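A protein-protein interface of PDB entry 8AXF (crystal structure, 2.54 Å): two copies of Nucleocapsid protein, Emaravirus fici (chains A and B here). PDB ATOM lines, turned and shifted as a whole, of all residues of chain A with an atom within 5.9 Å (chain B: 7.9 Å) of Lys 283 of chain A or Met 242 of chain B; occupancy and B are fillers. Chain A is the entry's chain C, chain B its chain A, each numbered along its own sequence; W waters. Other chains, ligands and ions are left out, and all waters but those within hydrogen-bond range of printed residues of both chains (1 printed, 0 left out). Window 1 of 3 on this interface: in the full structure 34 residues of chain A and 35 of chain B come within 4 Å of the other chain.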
ATOM      1  N   LYS A 223       3.282 -21.580 -27.004  1.00  0.00           N
ATOM      2  CA  LYS A 223       4.422 -20.690 -26.811  1.00  0.00           C
ATOM      3  C   LYS A 223       3.985 -19.232 -26.762  1.00  0.00           C
ATOM      4  O   LYS A 223       4.632 -18.415 -26.097  1.00  0.00           O
ATOM      5  CB  LYS A 223       5.454 -20.902 -27.921  1.00  0.00           C
ATOM      6  CG  LYS A 223       5.632 -22.355 -28.330  1.00  0.00           C
ATOM      7  CD  LYS A 223       7.026 -22.621 -28.873  1.00  0.00           C
ATOM      8  CE  LYS A 223       7.957 -23.090 -27.766  1.00  0.00           C
ATOM      9  NZ  LYS A 223       9.349 -23.310 -28.247  1.00  0.00           N
ATOM     10  N   ASN A 226       2.914 -18.667 -23.175  1.00  0.00           N
ATOM     11  CA  ASN A 226       3.965 -18.955 -22.198  1.00  0.00           C
ATOM     12  C   ASN A 226       3.714 -20.237 -21.411  1.00  0.00           C
ATOM     13  O   ASN A 226       4.214 -20.385 -20.291  1.00  0.00           O
ATOM     14  CB  ASN A 226       4.163 -17.784 -21.229  1.00  0.00           C
ATOM     15  CG  ASN A 226       4.595 -16.516 -21.932  1.00  0.00           C
ATOM     16  OD1 ASN A 226       5.044 -16.549 -23.077  1.00  0.00           O
ATOM     17  ND2 ASN A 226       4.470 -15.387 -21.245  1.00  0.00           N
ATOM     18  N   THR A 281       3.981 -12.396 -30.652  1.00  0.00           N
ATOM     19  CA  THR A 281       5.213 -12.427 -29.873  1.00  0.00           C
ATOM     20  C   THR A 281       4.907 -12.957 -28.476  1.00  0.00           C
ATOM     21  O   THR A 281       3.761 -12.939 -28.013  1.00  0.00           O
ATOM     22  CB  THR A 281       5.873 -11.045 -29.748  1.00  0.00           C
ATOM     23  OG1 THR A 281       5.200 -10.284 -28.740  1.00  0.00           O
ATOM     24  CG2 THR A 281       5.810 -10.278 -31.062  1.00  0.00           C
ATOM     25  N   SER A 282       5.955 -13.412 -27.795  1.00  0.00           N
ATOM     26  CA  SER A 282       5.842 -13.846 -26.406  1.00  0.00           C
ATOM     27  C   SER A 282       7.239 -13.892 -25.806  1.00  0.00           C
ATOM     28  O   SER A 282       8.242 -13.895 -26.526  1.00  0.00           O
ATOM     29  CB  SER A 282       5.149 -15.213 -26.266  1.00  0.00           C
ATOM     30  OG  SER A 282       6.034 -16.267 -26.597  1.00  0.00           O
ATOM     31  N   LYS A 283       7.299 -13.924 -24.469  1.00  0.00           N
ATOM     32  CA  LYS A 283       8.598 -14.045 -23.811  1.00  0.00           C
ATOM     33  C   LYS A 283       9.197 -15.424 -24.059  1.00  0.00           C
ATOM     34  O   LYS A 283      10.417 -15.569 -24.203  1.00  0.00           O
ATOM     35  CB  LYS A 283       8.480 -13.761 -22.311  1.00  0.00           C
ATOM     36  CG  LYS A 283       8.014 -14.937 -21.464  1.00  0.00           C
ATOM     37  CD  LYS A 283       8.771 -15.017 -20.134  1.00  0.00           C
ATOM     38  CE  LYS A 283       8.303 -13.961 -19.137  1.00  0.00           C
ATOM     39  NZ  LYS A 283       8.855 -14.191 -17.760  1.00  0.00           N
ATOM     40  N   THR A 284       8.344 -16.443 -24.159  1.00  0.00           N
ATOM     41  CA  THR A 284       8.831 -17.781 -24.458  1.00  0.00           C
ATOM     42  C   THR A 284       9.353 -17.868 -25.882  1.00  0.00           C
ATOM     43  O   THR A 284      10.343 -18.558 -26.152  1.00  0.00           O
ATOM     44  CB  THR A 284       7.725 -18.797 -24.241  1.00  0.00           C
ATOM     45  OG1 THR A 284       7.409 -18.884 -22.846  1.00  0.00           O
ATOM     46  CG2 THR A 284       8.177 -20.162 -24.737  1.00  0.00           C
ATOM     47  N   LYS A 285       8.702 -17.164 -26.808  1.00  0.00           N
ATOM     48  CA  LYS A 285       9.193 -17.127 -28.177  1.00  0.00           C
ATOM     49  C   LYS A 285      10.412 -16.222 -28.289  1.00  0.00           C
ATOM     50  O   LYS A 285      11.305 -16.474 -29.108  1.00  0.00           O
ATOM     51  CB  LYS A 285       8.092 -16.669 -29.122  1.00  0.00           C
ATOM     52  CG  LYS A 285       6.985 -17.697 -29.304  1.00  0.00           C
ATOM     53  CD  LYS A 285       5.765 -17.097 -29.972  1.00  0.00           C
ATOM     54  CE  LYS A 285       5.382 -17.877 -31.214  1.00  0.00           C
ATOM     55  NZ  LYS A 285       6.452 -17.811 -32.241  1.00  0.00           N
ATOM     56  N   ARG A 286      10.483 -15.168 -27.464  1.00  0.00           N
ATOM     57  CA  ARG A 286      11.679 -14.332 -27.455  1.00  0.00           C
ATOM     58  C   ARG A 286      12.848 -15.074 -26.816  1.00  0.00           C
ATOM     59  O   ARG A 286      13.996 -14.918 -27.245  1.00  0.00           O
ATOM     60  CB  ARG A 286      11.415 -13.012 -26.735  1.00  0.00           C
ATOM     61  CG  ARG A 286      10.655 -11.976 -27.555  1.00  0.00           C
ATOM     62  CD  ARG A 286      10.689 -10.609 -26.887  1.00  0.00           C
ATOM     63  NE  ARG A 286      10.055 -10.619 -25.571  1.00  0.00           N
ATOM     64  CZ  ARG A 286       8.754 -10.435 -25.366  1.00  0.00           C
ATOM     65  NH1 ARG A 286       7.940 -10.234 -26.396  1.00  0.00           N
ATOM     66  NH2 ARG A 286       8.263 -10.456 -24.134  1.00  0.00           N
ATOM     67  N   ASN A 287      12.574 -15.900 -25.800  1.00  0.00           N
ATOM     68  CA  ASN A 287      13.633 -16.705 -25.199  1.00  0.00           C
ATOM     69  C   ASN A 287      14.162 -17.732 -26.188  1.00  0.00           C
ATOM     70  O   ASN A 287      15.376 -17.945 -26.276  1.00  0.00           O
ATOM     71  CB  ASN A 287      13.127 -17.400 -23.937  1.00  0.00           C
ATOM     72  CG  ASN A 287      12.959 -16.450 -22.770  1.00  0.00           C
ATOM     73  OD1 ASN A 287      13.716 -15.493 -22.618  1.00  0.00           O
ATOM     74  ND2 ASN A 287      11.950 -16.704 -21.941  1.00  0.00           N
ATOM     75  N   ASP A 288      13.266 -18.381 -26.936  1.00  0.00           N
ATOM     76  CA  ASP A 288      13.693 -19.357 -27.935  1.00  0.00           C
ATOM     77  C   ASP A 288      14.579 -18.708 -28.990  1.00  0.00           C
ATOM     78  O   ASP A 288      15.617 -19.260 -29.374  1.00  0.00           O
ATOM     79  CB  ASP A 288      12.475 -20.011 -28.585  1.00  0.00           C
ATOM     80  CG  ASP A 288      11.685 -20.869 -27.618  1.00  0.00           C
ATOM     81  OD1 ASP A 288      12.277 -21.357 -26.633  1.00  0.00           O
ATOM     82  OD2 ASP A 288      10.472 -21.061 -27.847  1.00  0.00           O
ATOM     83  N   GLU B 201      21.643  -9.028 -14.299  1.00  0.00           N
ATOM     84  CA  GLU B 201      20.979  -8.666 -15.548  1.00  0.00           C
ATOM     85  C   GLU B 201      20.507  -7.217 -15.546  1.00  0.00           C
ATOM     86  O   GLU B 201      20.379  -6.609 -16.614  1.00  0.00           O
ATOM     87  CB  GLU B 201      19.800  -9.604 -15.811  1.00  0.00           C
ATOM     88  CG  GLU B 201      20.189 -11.045 -16.115  1.00  0.00           C
ATOM     89  CD  GLU B 201      20.057 -11.960 -14.911  1.00  0.00           C
ATOM     90  OE1 GLU B 201      20.287 -11.494 -13.776  1.00  0.00           O
ATOM     91  OE2 GLU B 201      19.714 -13.147 -15.101  1.00  0.00           O
ATOM     92  N   PHE B 202      20.298  -6.647 -14.369  1.00  0.00           N
ATOM     93  CA  PHE B 202      19.870  -5.233 -14.279  1.00  0.00           C
ATOM     94  C   PHE B 202      21.014  -4.323 -14.727  1.00  0.00           C
ATOM     95  O   PHE B 202      20.737  -3.230 -15.219  1.00  0.00           O
ATOM     96  CB  PHE B 202      19.371  -4.906 -12.873  1.00  0.00           C
ATOM     97  CG  PHE B 202      17.955  -5.308 -12.560  1.00  0.00           C
ATOM     98  CD1 PHE B 202      16.887  -4.581 -13.052  1.00  0.00           C
ATOM     99  CD2 PHE B 202      17.695  -6.397 -11.748  1.00  0.00           C
ATOM    100  CE1 PHE B 202      15.585  -4.943 -12.750  1.00  0.00           C
ATOM    101  CE2 PHE B 202      16.393  -6.762 -11.450  1.00  0.00           C
ATOM    102  CZ  PHE B 202      15.343  -6.034 -11.951  1.00  0.00           C
ATOM    103  N   TYR B 204      22.554  -4.538 -17.284  1.00  0.00           N
ATOM    104  CA  TYR B 204      22.503  -4.378 -18.734  1.00  0.00           C
ATOM    105  C   TYR B 204      22.259  -2.926 -19.125  1.00  0.00           C
ATOM    106  O   TYR B 204      22.671  -2.495 -20.208  1.00  0.00           O
ATOM    107  CB  TYR B 204      21.416  -5.279 -19.327  1.00  0.00           C
ATOM    108  CG  TYR B 204      21.405  -5.312 -20.839  1.00  0.00           C
ATOM    109  CD1 TYR B 204      22.170  -6.238 -21.536  1.00  0.00           C
ATOM    110  CD2 TYR B 204      20.632  -4.419 -21.572  1.00  0.00           C
ATOM    111  CE1 TYR B 204      22.168  -6.275 -22.918  1.00  0.00           C
ATOM    112  CE2 TYR B 204      20.625  -4.446 -22.953  1.00  0.00           C
ATOM    113  CZ  TYR B 204      21.395  -5.376 -23.621  1.00  0.00           C
ATOM    114  OH  TYR B 204      21.392  -5.409 -24.996  1.00  0.00           O
ATOM    115  N   ALA B 234      16.317 -21.788 -21.244  1.00  0.00           N
ATOM    116  CA  ALA B 234      15.425 -20.635 -21.273  1.00  0.00           C
ATOM    117  C   ALA B 234      15.441 -19.887 -19.946  1.00  0.00           C
ATOM    118  O   ALA B 234      15.419 -18.651 -19.923  1.00  0.00           O
ATOM    119  CB  ALA B 234      14.005 -21.077 -21.625  1.00  0.00           C
ATOM    120  N   VAL B 237      18.537 -17.526 -19.529  1.00  0.00           N
ATOM    121  CA  VAL B 237      18.569 -16.281 -20.289  1.00  0.00           C
ATOM    122  C   VAL B 237      17.309 -15.443 -20.127  1.00  0.00           C
ATOM    123  O   VAL B 237      17.288 -14.290 -20.590  1.00  0.00           O
ATOM    124  CB  VAL B 237      18.803 -16.554 -21.790  1.00  0.00           C
ATOM    125  CG1 VAL B 237      19.943 -17.538 -21.977  1.00  0.00           C
ATOM    126  CG2 VAL B 237      17.522 -17.065 -22.441  1.00  0.00           C
ATOM    127  N   SER B 238      16.266 -15.975 -19.485  1.00  0.00           N
ATOM    128  CA  SER B 238      14.967 -15.308 -19.465  1.00  0.00           C
ATOM    129  C   SER B 238      15.066 -13.893 -18.902  1.00  0.00           C
ATOM    130  O   SER B 238      14.584 -12.933 -19.513  1.00  0.00           O
ATOM    131  CB  SER B 238      13.970 -16.141 -18.656  1.00  0.00           C
ATOM    132  OG  SER B 238      12.640 -15.719 -18.895  1.00  0.00           O
ATOM    133  N   SER B 239      15.694 -13.746 -17.733  1.00  0.00           N
ATOM    134  CA  SER B 239      15.787 -12.414 -17.081  1.00  0.00           C
ATOM    135  C   SER B 239      16.465 -11.413 -18.017  1.00  0.00           C
ATOM    136  O   SER B 239      15.990 -10.280 -18.098  1.00  0.00           O
ATOM    137  CB  SER B 239      16.478 -12.465 -15.749  1.00  0.00           C
ATOM    138  OG  SER B 239      16.705 -11.162 -15.244  1.00  0.00           O
ATOM    139  N   LEU B 240      17.535 -11.830 -18.690  1.00  0.00           N
ATOM    140  CA  LEU B 240      18.235 -10.884 -19.557  1.00  0.00           C
ATOM    141  C   LEU B 240      17.376 -10.485 -20.748  1.00  0.00           C
ATOM    142  O   LEU B 240      17.347  -9.310 -21.136  1.00  0.00           O
ATOM    143  CB  LEU B 240      19.560 -11.475 -20.035  1.00  0.00           C
ATOM    144  CG  LEU B 240      20.226 -10.671 -21.157  1.00  0.00           C
ATOM    145  CD1 LEU B 240      20.690  -9.309 -20.659  1.00  0.00           C
ATOM    146  CD2 LEU B 240      21.375 -11.440 -21.774  1.00  0.00           C
ATOM    147  N   VAL B 241      16.677 -11.451 -21.350  1.00  0.00           N
ATOM    148  CA  VAL B 241      15.804 -11.151 -22.481  1.00  0.00           C
ATOM    149  C   VAL B 241      14.710 -10.174 -22.072  1.00  0.00           C
ATOM    150  O   VAL B 241      14.264  -9.353 -22.884  1.00  0.00           O
ATOM    151  CB  VAL B 241      15.225 -12.459 -23.059  1.00  0.00           C
ATOM    152  CG1 VAL B 241      14.266 -12.170 -24.202  1.00  0.00           C
ATOM    153  CG2 VAL B 241      16.350 -13.367 -23.528  1.00  0.00           C
ATOM    154  N   MET B 242      14.261 -10.250 -20.826  1.00  0.00           N
ATOM    155  CA  MET B 242      13.225  -9.304 -20.348  1.00  0.00           C
ATOM    156  C   MET B 242      13.803  -7.888 -20.340  1.00  0.00           C
ATOM    157  O   MET B 242      13.084  -6.964 -20.727  1.00  0.00           O
ATOM    158  CB  MET B 242      12.741  -9.680 -18.948  1.00  0.00           C
ATOM    159  CG  MET B 242      11.760 -10.826 -18.924  1.00  0.00           C
ATOM    160  SD  MET B 242      11.018 -11.028 -17.289  1.00  0.00           S
ATOM    161  CE  MET B 242      12.418 -10.661 -16.236  1.00  0.00           C
ATOM    162  N   LYS B 243      15.058  -7.738 -19.927  1.00  0.00           N
ATOM    163  CA  LYS B 243      15.714  -6.407 -19.873  1.00  0.00           C
ATOM    164  C   LYS B 243      16.009  -5.937 -21.293  1.00  0.00           C
ATOM    165  O   LYS B 243      15.839  -4.750 -21.559  1.00  0.00           O
ATOM    166  CB  LYS B 243      17.012  -6.457 -19.061  1.00  0.00           C
ATOM    167  CG  LYS B 243      16.989  -7.336 -17.823  1.00  0.00           C
ATOM    168  CD  LYS B 243      16.620  -6.601 -16.560  1.00  0.00           C
ATOM    169  CE  LYS B 243      16.383  -7.541 -15.400  1.00  0.00           C
ATOM    170  NZ  LYS B 243      15.141  -8.327 -15.583  1.00  0.00           N
ATOM    171  N   MET B 244      16.437  -6.848 -22.164  1.00  0.00           N
ATOM    172  CA  MET B 244      16.660  -6.471 -23.557  1.00  0.00           C
ATOM    173  C   MET B 244      15.359  -6.047 -24.226  1.00  0.00           C
ATOM    174  O   MET B 244      15.324  -5.042 -24.948  1.00  0.00           O
ATOM    175  CB  MET B 244      17.304  -7.628 -24.320  1.00  0.00           C
ATOM    176  CG  MET B 244      18.643  -8.084 -23.758  1.00  0.00           C
ATOM    177  SD  MET B 244      19.444  -9.341 -24.775  1.00  0.00           S
ATOM    178  CE  MET B 244      19.922  -8.371 -26.204  1.00  0.00           C
ATOM    179  N   ASN B 245      14.278  -6.797 -23.993  1.00  0.00           N
ATOM    180  CA  ASN B 245      12.991  -6.466 -24.596  1.00  0.00           C
ATOM    181  C   ASN B 245      12.505  -5.087 -24.167  1.00  0.00           C
ATOM    182  O   ASN B 245      11.861  -4.386 -24.953  1.00  0.00           O
ATOM    183  CB  ASN B 245      11.955  -7.527 -24.228  1.00  0.00           C
ATOM    184  CG  ASN B 245      10.592  -7.242 -24.823  1.00  0.00           C
ATOM    185  OD1 ASN B 245      10.469  -6.958 -26.014  1.00  0.00           O
ATOM    186  ND2 ASN B 245       9.559  -7.300 -23.990  1.00  0.00           N
ATOM    187  N   ARG B 246      12.804  -4.684 -22.940  1.00  0.00           N
ATOM    188  CA  ARG B 246      12.401  -3.339 -22.471  1.00  0.00           C
ATOM    189  C   ARG B 246      13.254  -2.285 -23.173  1.00  0.00           C
ATOM    190  O   ARG B 246      12.669  -1.339 -23.722  1.00  0.00           O
ATOM    191  CB  ARG B 246      12.541  -3.247 -20.951  1.00  0.00           C
ATOM    192  CG  ARG B 246      12.497  -1.832 -20.396  1.00  0.00           C
ATOM    193  CD  ARG B 246      12.914  -1.773 -18.939  1.00  0.00           C
ATOM    194  NE  ARG B 246      14.326  -2.067 -18.745  1.00  0.00           N
ATOM    195  CZ  ARG B 246      14.933  -2.089 -17.564  1.00  0.00           C
ATOM    196  NH1 ARG B 246      14.246  -1.832 -16.465  1.00  0.00           N
ATOM    197  NH2 ARG B 246      16.221  -2.367 -17.487  1.00  0.00           N
ATOM    198  N   ILE B 247      14.578  -2.453 -23.172  1.00  0.00           N
ATOM    199  CA  ILE B 247      15.463  -1.444 -23.744  1.00  0.00           C
ATOM    200  C   ILE B 247      15.261  -1.345 -25.252  1.00  0.00           C
ATOM    201  O   ILE B 247      15.068  -0.253 -25.797  1.00  0.00           O
ATOM    202  CB  ILE B 247      16.931  -1.758 -23.399  1.00  0.00           C
ATOM    203  CG1 ILE B 247      17.117  -1.942 -21.889  1.00  0.00           C
ATOM    204  CG2 ILE B 247      17.838  -0.660 -23.918  1.00  0.00           C
ATOM    205  CD1 ILE B 247      17.375  -0.661 -21.127  1.00  0.00           C
ATOM    206  N   HIS B 248      15.297  -2.483 -25.946  1.00  0.00           N
ATOM    207  CA  HIS B 248      15.333  -2.505 -27.403  1.00  0.00           C
ATOM    208  C   HIS B 248      13.960  -2.612 -28.057  1.00  0.00           C
ATOM    209  O   HIS B 248      13.857  -2.390 -29.268  1.00  0.00           O
ATOM    210  CB  HIS B 248      16.197  -3.673 -27.897  1.00  0.00           C
ATOM    211  CG  HIS B 248      17.614  -3.633 -27.414  1.00  0.00           C
ATOM    212  ND1 HIS B 248      18.589  -2.875 -28.027  1.00  0.00           N
ATOM    213  CD2 HIS B 248      18.224  -4.272 -26.388  1.00  0.00           C
ATOM    214  CE1 HIS B 248      19.736  -3.040 -27.394  1.00  0.00           C
ATOM    215  NE2 HIS B 248      19.542  -3.884 -26.396  1.00  0.00           N
ATOM    216  N   LYS B 249      12.913  -2.947 -27.298  1.00  0.00           N
ATOM    217  CA  LYS B 249      11.596  -3.271 -27.849  1.00  0.00           C
ATOM    218  C   LYS B 249      11.696  -4.433 -28.841  1.00  0.00           C
ATOM    219  O   LYS B 249      11.448  -4.294 -30.041  1.00  0.00           O
ATOM    220  CB  LYS B 249      10.937  -2.042 -28.484  1.00  0.00           C
ATOM    221  CG  LYS B 249      10.041  -1.275 -27.524  1.00  0.00           C
ATOM    222  CD  LYS B 249       8.749  -2.033 -27.255  1.00  0.00           C
ATOM    223  CE  LYS B 249       8.091  -1.593 -25.954  1.00  0.00           C
ATOM    224  NZ  LYS B 249       8.523  -2.424 -24.792  1.00  0.00           N
ATOM    225  N   LEU B 250      12.053  -5.602 -28.301  1.00  0.00           N
ATOM    226  CA  LEU B 250      12.292  -6.791 -29.112  1.00  0.00           C
ATOM    227  C   LEU B 250      11.057  -7.264 -29.870  1.00  0.00           C
ATOM    228  O   LEU B 250      11.184  -8.138 -30.735  1.00  0.00           O
ATOM    229  CB  LEU B 250      12.814  -7.931 -28.233  1.00  0.00           C
ATOM    230  CG  LEU B 250      14.240  -7.814 -27.693  1.00  0.00           C
ATOM    231  CD1 LEU B 250      14.577  -9.015 -26.827  1.00  0.00           C
ATOM    232  CD2 LEU B 250      15.230  -7.690 -28.828  1.00  0.00           C
ATOM    233  N   GLU B 251       9.873  -6.726 -29.566  1.00  0.00           N
ATOM    234  CA  GLU B 251       8.682  -7.098 -30.325  1.00  0.00           C
ATOM    235  C   GLU B 251       8.738  -6.546 -31.743  1.00  0.00           C
ATOM    236  O   GLU B 251       8.277  -7.195 -32.689  1.00  0.00           O
ATOM    237  CB  GLU B 251       7.429  -6.611 -29.599  1.00  0.00           C
ATOM    238  CG  GLU B 251       7.195  -7.292 -28.259  1.00  0.00           C
ATOM    239  CD  GLU B 251       6.773  -6.321 -27.175  1.00  0.00           C
ATOM    240  OE1 GLU B 251       6.825  -5.097 -27.418  1.00  0.00           O
ATOM    241  OE2 GLU B 251       6.396  -6.780 -26.076  1.00  0.00           O
ATOM    242  N   PHE B 255      17.053  -9.165 -32.824  1.00  0.00           N
ATOM    243  CA  PHE B 255      18.175  -9.402 -31.924  1.00  0.00           C
ATOM    244  C   PHE B 255      19.476  -8.900 -32.537  1.00  0.00           C
ATOM    245  O   PHE B 255      20.302  -8.293 -31.846  1.00  0.00           O
ATOM    246  CB  PHE B 255      18.278 -10.887 -31.582  1.00  0.00           C
ATOM    247  CG  PHE B 255      17.457 -11.293 -30.393  1.00  0.00           C
ATOM    248  CD1 PHE B 255      17.953 -11.138 -29.110  1.00  0.00           C
ATOM    249  CD2 PHE B 255      16.191 -11.832 -30.558  1.00  0.00           C
ATOM    250  CE1 PHE B 255      17.201 -11.511 -28.012  1.00  0.00           C
ATOM    251  CE2 PHE B 255      15.436 -12.206 -29.464  1.00  0.00           C
ATOM    252  CZ  PHE B 255      15.941 -12.047 -28.190  1.00  0.00           C
HETATM  253  O   HOH W   1      12.238 -13.172 -21.633  1.00  0.00           O
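Of chain B, only Met 242 (3.9 Å) comes within 4 Å of Lys 283 of chain A.
Of chain A, only Lys 283 (3.9 Å) comes within 4 Å of Met 242 of chain B.
Of the printed residues of chain A, Ser 238 of chain B touches Asn 287 (3.3 Å).
Printed residues of chain A within 4 Å of Glu 251 of chain B: Thr 281 and Arg 286.
Lys 243 of chain B touches none of the printed residues of chain A.
Glu 201 of chain B touches none of the printed residues of chain A.
The nearest residue of chain B that does not touch Lys 283 of chain A is Ser 238 of chain B (4.1 Å).
The backbone NH (N) of Leu 250 of chain B is in hydrogen-bond range of the side-chain amide oxygen (OD1) of Asn 245 of chain B.
The side-chain amide nitrogen of Asn 287 of chain A lies within hydrogen-bond range of the backbone carbonyl oxygen of Lys 283 of chain A.
No position is printed for both chains.
Printed residues of chain B that touch a printed residue of chain A: Ser 238, Val 241, Met 242, Asn 245, Leu 250, Glu 251 and Phe 255.
Hydrophobic or aromatic side chains of chain B within 4 Å of the printed part of chain A: Val 241, Met 242, Leu 250 and Phe 255.
Among the printed residues, Asp or Glu carboxylates within 4 Å of a Lys or Arg side-chain nitrogen of the other chain: Arg 286 of chain A with Glu 251 of chain B.
Among the printed residues, pairs that only touch across the chains: Thr 281 of chain A with Glu 251 of chain B (3.6 Å), Lys 283 of chain A with Met 242 of chain B (3.9 Å), Arg 286 of chain A with Val 241 of chain B (3.9 Å), Arg 286 of chain A with Leu 250 of chain B (3.7 Å), Arg 286 of chain A with Phe 255 of chain B (3.6 Å) and Asn 287 of chain A with Val 241 of chain B (3.4 Å).
The side-chain hydroxyl of Ser 238 of chain B is in hydrogen-bond range of the side-chain amide nitrogen of Asn 287 of chain A, 3.3 Å away.
NH2 of Arg 286 of chain A sits close to ND2 of Asn 245 of chain B.
The guanidinium group (NH1) of Arg 286 of chain A lies within salt-bridge range of the side-chain carboxylate (OE2) of Glu 251 of chain B.
Water W1 bridges OD1 of Asn 287 of chain A (2.9 Å) and O of Ser 238 of chain B (3.2 Å).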
